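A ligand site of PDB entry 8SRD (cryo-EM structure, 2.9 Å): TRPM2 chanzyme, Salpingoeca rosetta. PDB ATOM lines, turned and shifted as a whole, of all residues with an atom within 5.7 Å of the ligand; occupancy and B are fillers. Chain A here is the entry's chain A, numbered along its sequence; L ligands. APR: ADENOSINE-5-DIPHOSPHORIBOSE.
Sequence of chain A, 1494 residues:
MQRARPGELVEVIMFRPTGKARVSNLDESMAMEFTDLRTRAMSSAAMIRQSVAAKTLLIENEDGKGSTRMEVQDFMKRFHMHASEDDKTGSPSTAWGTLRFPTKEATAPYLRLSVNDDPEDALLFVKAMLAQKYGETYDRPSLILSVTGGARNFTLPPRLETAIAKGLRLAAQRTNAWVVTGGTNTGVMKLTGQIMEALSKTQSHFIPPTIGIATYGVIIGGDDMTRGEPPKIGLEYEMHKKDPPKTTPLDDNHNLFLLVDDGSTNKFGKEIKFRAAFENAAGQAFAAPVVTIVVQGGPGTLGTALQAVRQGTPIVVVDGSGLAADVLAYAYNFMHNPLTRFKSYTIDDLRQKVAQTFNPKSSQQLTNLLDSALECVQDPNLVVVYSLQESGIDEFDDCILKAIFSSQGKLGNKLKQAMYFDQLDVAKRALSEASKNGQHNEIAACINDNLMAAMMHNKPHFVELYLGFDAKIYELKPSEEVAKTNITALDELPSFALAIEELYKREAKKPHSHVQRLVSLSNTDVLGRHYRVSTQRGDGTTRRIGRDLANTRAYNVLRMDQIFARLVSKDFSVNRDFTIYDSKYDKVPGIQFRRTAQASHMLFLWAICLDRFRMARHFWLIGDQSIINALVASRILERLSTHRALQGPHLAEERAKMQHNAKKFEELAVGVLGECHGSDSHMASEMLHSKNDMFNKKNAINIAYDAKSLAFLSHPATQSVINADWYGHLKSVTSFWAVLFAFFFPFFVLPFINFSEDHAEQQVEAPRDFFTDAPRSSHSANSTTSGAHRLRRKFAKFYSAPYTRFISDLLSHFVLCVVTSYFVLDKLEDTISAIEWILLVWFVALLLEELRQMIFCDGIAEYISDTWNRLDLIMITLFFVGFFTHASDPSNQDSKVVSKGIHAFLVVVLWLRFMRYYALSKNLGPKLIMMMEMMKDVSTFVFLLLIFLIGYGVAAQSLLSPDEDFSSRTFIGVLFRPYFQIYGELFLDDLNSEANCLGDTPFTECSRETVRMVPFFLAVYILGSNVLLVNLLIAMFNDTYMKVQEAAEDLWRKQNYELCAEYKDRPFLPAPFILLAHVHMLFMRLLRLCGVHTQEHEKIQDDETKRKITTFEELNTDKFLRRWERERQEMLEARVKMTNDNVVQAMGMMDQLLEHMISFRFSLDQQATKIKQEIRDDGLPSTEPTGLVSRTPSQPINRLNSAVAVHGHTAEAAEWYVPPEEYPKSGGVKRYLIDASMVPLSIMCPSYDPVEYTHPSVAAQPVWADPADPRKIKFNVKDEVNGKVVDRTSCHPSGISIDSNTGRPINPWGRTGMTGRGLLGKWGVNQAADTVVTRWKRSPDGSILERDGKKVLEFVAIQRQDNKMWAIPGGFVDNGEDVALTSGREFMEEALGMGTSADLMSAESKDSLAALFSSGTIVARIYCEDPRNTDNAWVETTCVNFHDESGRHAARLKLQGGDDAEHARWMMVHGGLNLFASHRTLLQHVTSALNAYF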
ATOM      1  N   VAL A 147     -27.215  14.520  29.419  1.00  0.00           N
ATOM      2  CA  VAL A 147     -28.302  15.283  30.039  1.00  0.00           C
ATOM      3  C   VAL A 147     -28.444  16.607  29.285  1.00  0.00           C
ATOM      4  O   VAL A 147     -27.516  17.424  29.293  1.00  0.00           O
ATOM      5  CB  VAL A 147     -28.092  15.512  31.540  1.00  0.00           C
ATOM      6  CG1 VAL A 147     -29.358  16.082  32.141  1.00  0.00           C
ATOM      7  CG2 VAL A 147     -27.806  14.194  32.220  1.00  0.00           C
ATOM      8  N   THR A 148     -29.580  16.809  28.634  1.00  0.00           N
ATOM      9  CA  THR A 148     -29.858  18.049  27.916  1.00  0.00           C
ATOM     10  C   THR A 148     -31.184  18.653  28.361  1.00  0.00           C
ATOM     11  O   THR A 148     -32.015  17.991  28.995  1.00  0.00           O
ATOM     12  CB  THR A 148     -29.873  17.845  26.390  1.00  0.00           C
ATOM     13  OG1 THR A 148     -30.116  19.109  25.753  1.00  0.00           O
ATOM     14  CG2 THR A 148     -30.946  16.872  25.960  1.00  0.00           C
ATOM     15  N   GLY A 149     -31.359  19.936  28.054  1.00  0.00           N
ATOM     16  CA  GLY A 149     -32.607  20.612  28.339  1.00  0.00           C
ATOM     17  C   GLY A 149     -32.486  22.115  28.473  1.00  0.00           C
ATOM     18  O   GLY A 149     -31.664  22.759  27.815  1.00  0.00           O
ATOM     19  N   GLY A 150     -33.380  22.663  29.316  1.00  0.00           N
ATOM     20  CA  GLY A 150     -33.525  24.110  29.423  1.00  0.00           C
ATOM     21  C   GLY A 150     -32.373  24.828  30.101  1.00  0.00           C
ATOM     22  O   GLY A 150     -31.963  24.496  31.212  1.00  0.00           O
ATOM     23  N   ALA A 151     -31.877  25.897  29.487  1.00  0.00           N
ATOM     24  CA  ALA A 151     -30.807  26.663  30.164  1.00  0.00           C
ATOM     25  C   ALA A 151     -31.374  27.754  31.055  1.00  0.00           C
ATOM     26  O   ALA A 151     -31.369  27.550  32.275  1.00  0.00           O
ATOM     27  CB  ALA A 151     -29.913  27.250  29.126  1.00  0.00           C
ATOM     28  N   ARG A 152     -31.897  28.831  30.490  1.00  0.00           N
ATOM     29  CA  ARG A 152     -32.329  30.012  31.221  1.00  0.00           C
ATOM     30  C   ARG A 152     -33.799  29.853  31.574  1.00  0.00           C
ATOM     31  O   ARG A 152     -34.269  30.483  32.520  1.00  0.00           O
ATOM     32  CB  ARG A 152     -32.070  31.334  30.488  1.00  0.00           C
ATOM     33  CG  ARG A 152     -30.712  31.361  29.807  1.00  0.00           C
ATOM     34  CD  ARG A 152     -30.349  32.768  29.299  1.00  0.00           C
ATOM     35  NE  ARG A 152     -30.139  33.750  30.358  1.00  0.00           N
ATOM     36  CZ  ARG A 152     -29.054  33.881  31.129  1.00  0.00           C
ATOM     37  NH1 ARG A 152     -27.994  33.095  30.994  1.00  0.00           N
ATOM     38  NH2 ARG A 152     -29.029  34.831  32.055  1.00  0.00           N
ATOM     39  N   ASN A 153     -34.536  29.033  30.825  1.00  0.00           N
ATOM     40  CA  ASN A 153     -35.962  28.870  31.073  1.00  0.00           C
ATOM     41  C   ASN A 153     -36.208  27.563  31.838  1.00  0.00           C
ATOM     42  O   ASN A 153     -37.146  26.809  31.538  1.00  0.00           O
ATOM     43  CB  ASN A 153     -36.711  28.947  29.731  1.00  0.00           C
ATOM     44  CG  ASN A 153     -38.195  29.306  29.889  1.00  0.00           C
ATOM     45  OD1 ASN A 153     -38.685  29.500  31.002  1.00  0.00           O
ATOM     46  ND2 ASN A 153     -38.894  29.417  28.762  1.00  0.00           N
ATOM     47  N   PHE A 154     -35.347  27.248  32.799  1.00  0.00           N
ATOM     48  CA  PHE A 154     -35.517  26.058  33.627  1.00  0.00           C
ATOM     49  C   PHE A 154     -36.005  26.466  35.020  1.00  0.00           C
ATOM     50  O   PHE A 154     -35.239  26.609  35.972  1.00  0.00           O
ATOM     51  CB  PHE A 154     -34.235  25.241  33.681  1.00  0.00           C
ATOM     52  CG  PHE A 154     -34.436  23.841  34.163  1.00  0.00           C
ATOM     53  CD1 PHE A 154     -34.802  22.843  33.263  1.00  0.00           C
ATOM     54  CD2 PHE A 154     -34.199  23.507  35.516  1.00  0.00           C
ATOM     55  CE1 PHE A 154     -35.010  21.536  33.694  1.00  0.00           C
ATOM     56  CE2 PHE A 154     -34.381  22.199  35.968  1.00  0.00           C
ATOM     57  CZ  PHE A 154     -34.781  21.205  35.051  1.00  0.00           C
ATOM     58  N   GLY A 182     -24.193  20.311  28.508  1.00  0.00           N
ATOM     59  CA  GLY A 182     -23.659  21.546  27.967  1.00  0.00           C
ATOM     60  C   GLY A 182     -22.606  22.064  28.932  1.00  0.00           C
ATOM     61  O   GLY A 182     -22.610  21.746  30.113  1.00  0.00           O
ATOM     62  N   THR A 184     -22.390  25.055  30.211  1.00  0.00           N
ATOM     63  CA  THR A 184     -22.756  26.321  30.872  1.00  0.00           C
ATOM     64  C   THR A 184     -23.208  26.207  32.321  1.00  0.00           C
ATOM     65  O   THR A 184     -23.524  25.101  32.749  1.00  0.00           O
ATOM     66  CB  THR A 184     -23.681  27.110  29.960  1.00  0.00           C
ATOM     67  OG1 THR A 184     -24.905  26.373  29.850  1.00  0.00           O
ATOM     68  CG2 THR A 184     -23.097  27.335  28.589  1.00  0.00           C
ATOM     69  N   THR A 186     -25.892  27.286  33.913  1.00  0.00           N
ATOM     70  CA  THR A 186     -27.309  27.692  33.850  1.00  0.00           C
ATOM     71  C   THR A 186     -28.223  26.479  33.782  1.00  0.00           C
ATOM     72  O   THR A 186     -27.936  25.582  32.997  1.00  0.00           O
ATOM     73  CB  THR A 186     -27.532  28.455  32.540  1.00  0.00           C
ATOM     74  OG1 THR A 186     -27.197  27.573  31.467  1.00  0.00           O
ATOM     75  CG2 THR A 186     -26.728  29.725  32.438  1.00  0.00           C
ATOM     76  N   VAL A 188     -30.439  23.064  34.084  1.00  0.00           N
ATOM     77  CA  VAL A 188     -30.398  21.603  34.295  1.00  0.00           C
ATOM     78  C   VAL A 188     -28.979  21.047  34.280  1.00  0.00           C
ATOM     79  O   VAL A 188     -28.683  20.124  35.077  1.00  0.00           O
ATOM     80  CB  VAL A 188     -31.385  20.893  33.300  1.00  0.00           C
ATOM     81  CG1 VAL A 188     -30.954  20.886  31.817  1.00  0.00           C
ATOM     82  CG2 VAL A 188     -31.741  19.475  33.766  1.00  0.00           C
ATOM     83  N   MET A 189     -28.081  21.675  33.496  1.00  0.00           N
ATOM     84  CA  MET A 189     -26.648  21.368  33.403  1.00  0.00           C
ATOM     85  C   MET A 189     -25.968  21.628  34.736  1.00  0.00           C
ATOM     86  O   MET A 189     -25.241  20.748  35.238  1.00  0.00           O
ATOM     87  CB  MET A 189     -25.993  22.142  32.264  1.00  0.00           C
ATOM     88  CG  MET A 189     -26.670  21.914  30.916  1.00  0.00           C
ATOM     89  SD  MET A 189     -26.498  23.232  29.693  1.00  0.00           S
ATOM     90  CE  MET A 189     -27.834  24.310  30.135  1.00  0.00           C
ATOM     91  N   ILE A 213     -19.887  20.410  26.720  1.00  0.00           N
ATOM     92  CA  ILE A 213     -19.702  20.866  25.343  1.00  0.00           C
ATOM     93  C   ILE A 213     -20.439  22.193  25.169  1.00  0.00           C
ATOM     94  O   ILE A 213     -21.674  22.229  25.234  1.00  0.00           O
ATOM     95  CB  ILE A 213     -20.199  19.821  24.347  1.00  0.00           C
ATOM     96  CG1 ILE A 213     -19.512  18.469  24.598  1.00  0.00           C
ATOM     97  CG2 ILE A 213     -19.971  20.315  22.935  1.00  0.00           C
ATOM     98  CD1 ILE A 213     -19.908  17.367  23.639  1.00  0.00           C
ATOM     99  N   THR A 248     -22.947  34.365  29.482  1.00  0.00           N
ATOM    100  CA  THR A 248     -23.107  32.990  29.973  1.00  0.00           C
ATOM    101  C   THR A 248     -21.791  32.377  30.461  1.00  0.00           C
ATOM    102  O   THR A 248     -20.895  32.156  29.628  1.00  0.00           O
ATOM    103  CB  THR A 248     -23.736  32.116  28.896  1.00  0.00           C
ATOM    104  OG1 THR A 248     -22.988  32.294  27.693  1.00  0.00           O
ATOM    105  CG2 THR A 248     -25.170  32.539  28.638  1.00  0.00           C
ATOM    106  N   PHE A 268     -26.109  30.914  19.966  1.00  0.00           N
ATOM    107  CA  PHE A 268     -26.103  29.492  20.392  1.00  0.00           C
ATOM    108  C   PHE A 268     -26.808  28.616  19.355  1.00  0.00           C
ATOM    109  O   PHE A 268     -27.542  29.197  18.541  1.00  0.00           O
ATOM    110  CB  PHE A 268     -26.930  29.344  21.668  1.00  0.00           C
ATOM    111  CG  PHE A 268     -26.680  30.339  22.780  1.00  0.00           C
ATOM    112  CD1 PHE A 268     -27.223  31.607  22.732  1.00  0.00           C
ATOM    113  CD2 PHE A 268     -25.959  29.968  23.892  1.00  0.00           C
ATOM    114  CE1 PHE A 268     -27.001  32.509  23.762  1.00  0.00           C
ATOM    115  CE2 PHE A 268     -25.745  30.873  24.928  1.00  0.00           C
ATOM    116  CZ  PHE A 268     -26.268  32.134  24.855  1.00  0.00           C
ATOM    117  N   GLY A 269     -26.502  27.320  19.426  1.00  0.00           N
ATOM    118  CA  GLY A 269     -27.094  26.335  18.497  1.00  0.00           C
ATOM    119  C   GLY A 269     -26.035  25.773  17.587  1.00  0.00           C
ATOM    120  O   GLY A 269     -26.400  25.106  16.615  1.00  0.00           O
ATOM    121  N   GLU A 271     -23.455  23.693  18.399  1.00  0.00           N
ATOM    122  CA  GLU A 271     -22.751  22.466  18.852  1.00  0.00           C
ATOM    123  C   GLU A 271     -23.680  21.272  18.749  1.00  0.00           C
ATOM    124  O   GLU A 271     -23.201  20.155  18.955  1.00  0.00           O
ATOM    125  CB  GLU A 271     -22.387  22.628  20.322  1.00  0.00           C
ATOM    126  CG  GLU A 271     -23.495  22.248  21.286  1.00  0.00           C
ATOM    127  CD  GLU A 271     -24.183  23.423  21.973  1.00  0.00           C
ATOM    128  OE1 GLU A 271     -24.276  24.489  21.343  1.00  0.00           O
ATOM    129  OE2 GLU A 271     -24.627  23.245  23.122  1.00  0.00           O
ATOM    130  N   ILE A 272     -24.961  21.464  18.486  1.00  0.00           N
ATOM    131  CA  ILE A 272     -25.891  20.307  18.534  1.00  0.00           C
ATOM    132  C   ILE A 272     -25.336  19.130  17.718  1.00  0.00           C
ATOM    133  O   ILE A 272     -25.221  18.046  18.297  1.00  0.00           O
ATOM    134  CB  ILE A 272     -27.277  20.783  18.103  1.00  0.00           C
ATOM    135  CG1 ILE A 272     -27.880  21.719  19.134  1.00  0.00           C
ATOM    136  CG2 ILE A 272     -28.181  19.598  17.816  1.00  0.00           C
ATOM    137  CD1 ILE A 272     -28.853  22.720  18.562  1.00  0.00           C
ATOM    138  N   ARG A 275     -22.130  17.575  19.197  1.00  0.00           N
ATOM    139  CA  ARG A 275     -22.449  16.867  20.447  1.00  0.00           C
ATOM    140  C   ARG A 275     -23.040  15.488  20.186  1.00  0.00           C
ATOM    141  O   ARG A 275     -22.597  14.510  20.797  1.00  0.00           O
ATOM    142  CB  ARG A 275     -23.394  17.698  21.325  1.00  0.00           C
ATOM    143  CG  ARG A 275     -23.726  17.078  22.675  1.00  0.00           C
ATOM    144  CD  ARG A 275     -24.677  17.914  23.500  1.00  0.00           C
ATOM    145  NE  ARG A 275     -25.292  17.117  24.541  1.00  0.00           N
ATOM    146  CZ  ARG A 275     -26.023  17.608  25.539  1.00  0.00           C
ATOM    147  NH1 ARG A 275     -26.252  18.905  25.648  1.00  0.00           N
ATOM    148  NH2 ARG A 275     -26.529  16.769  26.442  1.00  0.00           N
ATOM    149  N   GLY A 297     -36.910  22.059  28.415  1.00  0.00           N
ATOM    150  CA  GLY A 297     -36.314  22.212  27.088  1.00  0.00           C
ATOM    151  C   GLY A 297     -36.757  23.458  26.365  1.00  0.00           C
ATOM    152  O   GLY A 297     -37.653  24.134  26.848  1.00  0.00           O
ATOM    153  N   GLY A 298     -36.125  23.728  25.236  1.00  0.00           N
ATOM    154  CA  GLY A 298     -36.440  24.900  24.426  1.00  0.00           C
ATOM    155  C   GLY A 298     -36.104  24.516  23.015  1.00  0.00           C
ATOM    156  O   GLY A 298     -35.902  23.322  22.797  1.00  0.00           O
ATOM    157  N   PRO A 299     -36.004  25.416  22.027  1.00  0.00           N
ATOM    158  CA  PRO A 299     -35.810  24.951  20.621  1.00  0.00           C
ATOM    159  C   PRO A 299     -34.545  24.160  20.319  1.00  0.00           C
ATOM    160  O   PRO A 299     -34.548  23.274  19.445  1.00  0.00           O
ATOM    161  CB  PRO A 299     -35.832  26.268  19.825  1.00  0.00           C
ATOM    162  CG  PRO A 299     -36.542  27.227  20.674  1.00  0.00           C
ATOM    163  CD  PRO A 299     -36.216  26.873  22.079  1.00  0.00           C
ATOM    164  N   GLY A 300     -33.426  24.500  20.990  1.00  0.00           N
ATOM    165  CA  GLY A 300     -32.191  23.761  20.764  1.00  0.00           C
ATOM    166  C   GLY A 300     -32.198  22.368  21.368  1.00  0.00           C
ATOM    167  O   GLY A 300     -31.429  21.506  20.923  1.00  0.00           O
ATOM    168  N   THR A 301     -33.002  22.166  22.420  1.00  0.00           N
ATOM    169  CA  THR A 301     -33.194  20.834  23.010  1.00  0.00           C
ATOM    170  C   THR A 301     -33.920  19.899  22.036  1.00  0.00           C
ATOM    171  O   THR A 301     -33.618  18.700  21.939  1.00  0.00           O
ATOM    172  CB  THR A 301     -33.936  21.041  24.329  1.00  0.00           C
ATOM    173  OG1 THR A 301     -33.086  21.772  25.215  1.00  0.00           O
ATOM    174  CG2 THR A 301     -34.304  19.768  25.038  1.00  0.00           C
ATOM    175  N   THR A 304     -31.384  19.041  19.502  1.00  0.00           N
ATOM    176  CA  THR A 304     -30.510  18.046  20.151  1.00  0.00           C
ATOM    177  C   THR A 304     -31.100  16.647  20.082  1.00  0.00           C
ATOM    178  O   THR A 304     -30.400  15.680  19.713  1.00  0.00           O
ATOM    179  CB  THR A 304     -30.243  18.493  21.601  1.00  0.00           C
ATOM    180  OG1 THR A 304     -29.513  19.725  21.585  1.00  0.00           O
ATOM    181  CG2 THR A 304     -29.440  17.478  22.409  1.00  0.00           C
HETATM  182  N1  APR L   1     -26.391  27.624  27.663  1.00  0.00           N
HETATM  183  C2  APR L   1     -26.869  28.759  28.195  1.00  0.00           C
HETATM  184  N3  APR L   1     -27.834  29.494  27.627  1.00  0.00           N
HETATM  185  C4  APR L   1     -28.371  29.120  26.455  1.00  0.00           C
HETATM  186  C5  APR L   1     -27.894  27.893  25.804  1.00  0.00           C
HETATM  187  C6  APR L   1     -26.841  27.145  26.498  1.00  0.00           C
HETATM  188  N6  APR L   1     -26.334  26.009  25.973  1.00  0.00           N
HETATM  189  N7  APR L   1     -28.594  27.764  24.670  1.00  0.00           N
HETATM  190  C8  APR L   1     -29.442  28.817  24.594  1.00  0.00           C
HETATM  191  N9  APR L   1     -29.299  29.621  25.662  1.00  0.00           N
HETATM  192  C1' APR L   1     -30.055  30.846  25.935  1.00  0.00           C
HETATM  193  C2' APR L   1     -30.699  31.344  24.667  1.00  0.00           C
HETATM  194  O2' APR L   1     -30.230  32.659  24.404  1.00  0.00           O
HETATM  195  C3' APR L   1     -32.179  31.412  24.938  1.00  0.00           C
HETATM  196  O3' APR L   1     -32.619  32.752  24.728  1.00  0.00           O
HETATM  197  O4' APR L   1     -31.102  30.498  26.817  1.00  0.00           O
HETATM  198  C4' APR L   1     -32.333  31.080  26.403  1.00  0.00           C
HETATM  199  C5' APR L   1     -33.441  30.079  26.623  1.00  0.00           C
HETATM  200  O5' APR L   1     -32.929  28.786  26.344  1.00  0.00           O
HETATM  201  PA  APR L   1     -33.689  27.537  26.975  1.00  0.00           P
HETATM  202  O1A APR L   1     -33.712  27.737  28.462  1.00  0.00           O
HETATM  203  O2A APR L   1     -34.980  27.353  26.228  1.00  0.00           O
HETATM  204  O3A APR L   1     -32.699  26.331  26.643  1.00  0.00           O
HETATM  205  PB  APR L   1     -32.623  25.781  25.148  1.00  0.00           P
HETATM  206  O1B APR L   1     -33.010  26.841  24.158  1.00  0.00           O
HETATM  207  O2B APR L   1     -33.269  24.437  25.112  1.00  0.00           O
HETATM  208  O5D APR L   1     -31.071  25.502  24.966  1.00  0.00           O
HETATM  209  C5D APR L   1     -30.714  24.354  24.215  1.00  0.00           C
HETATM  210  O4D APR L   1     -29.289  23.567  25.969  1.00  0.00           O
HETATM  211  O1D APR L   1     -29.199  21.509  27.012  1.00  0.00           O
HETATM  212  C1D APR L   1     -28.513  22.388  26.130  1.00  0.00           C
HETATM  213  O2D APR L   1     -27.019  21.486  24.467  1.00  0.00           O
HETATM  214  C2D APR L   1     -28.386  21.753  24.769  1.00  0.00           C
HETATM  215  O3D APR L   1     -27.760  23.153  22.948  1.00  0.00           O
HETATM  216  C3D APR L   1     -28.858  22.785  23.781  1.00  0.00           C
HETATM  217  C4D APR L   1     -29.311  23.960  24.602  1.00  0.00           C
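Gly 150 touches the ligand (C to O1A, 3.6 Å). Thr 186 touches the ligand. CE1 of Phe 268 touches O2' of the ligand, at 3.3 Å. Gly 297 touches the ligand (C to O2B, 3.8 Å). Pro 299 touches the ligand (CD to O1B, 3.8 Å). Gly 300 touches the ligand. OG1 of Thr 304 touches C3D of the ligand, 3.8 Å away. Hydrophobic or aromatic side chains that line the ligand: Ala 151, Phe 268 and Pro 299. Of the 26 residues printed, 17 come within 4 Å of the ligand. Along chain A the residues within 4 Å of the ligand span positions 148 to 304.
The side-chain hydroxyl (OG1) of Thr 184 lies within hydrogen-bond range of the side-chain hydroxyl (OG1) of Thr 186 (3.1 Å). The side-chain hydroxyl (OG1) of Thr 184 lies within hydrogen-bond range of the side-chain sulfur (SD) of Met 189 (3.5 Å). The guanidinium group of Arg 275 lies within hydrogen-bond range of the backbone carbonyl oxygen of Val 147, 3.1 Å away. The backbone carbonyl oxygen (O) of Gly 149 is in hydrogen-bond range of the side-chain hydroxyl (OG1) of Thr 301 (3.1 Å). OG1 of Thr 304 sits at hydrogen-bond distance from O of Gly 300.
The backbone NH (N) of Asn 153 is in hydrogen-bond range of an oxygen (O1A) of the ligand. The side-chain carboxylate of Glu 271 lies within hydrogen-bond range of an oxygen (O3D) of the ligand (3.1 Å). O2B of the ligand sits at hydrogen-bond distance from N of Gly 298 (2.9 Å). An oxygen (O1D) of the ligand sits at hydrogen-bond distance from the side-chain hydroxyl of Thr 148, 2.9 Å away. N of Ala 151 sits at hydrogen-bond distance from O1A of the ligand. O2D of the ligand lies within hydrogen-bond range of NH1 of Arg 275, 2.9 Å away. The side-chain hydroxyl (OG1) of Thr 301 lies within hydrogen-bond range of an oxygen (O2B) of the ligand, at 2.7 Å. An oxygen (O1A) of the ligand sits at hydrogen-bond distance from the backbone NH (N) of Arg 152, at 2.9 Å. The side-chain hydroxyl (OG1) of Thr 184 is in hydrogen-bond range of a nitrogen (N1) of the ligand. An oxygen (O1D) of the ligand sits at hydrogen-bond distance from the backbone carbonyl oxygen (O) of Gly 149 (2.9 Å). N of Gly 149 is in hydrogen-bond range of O1D of the ligand, 2.9 Å away.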
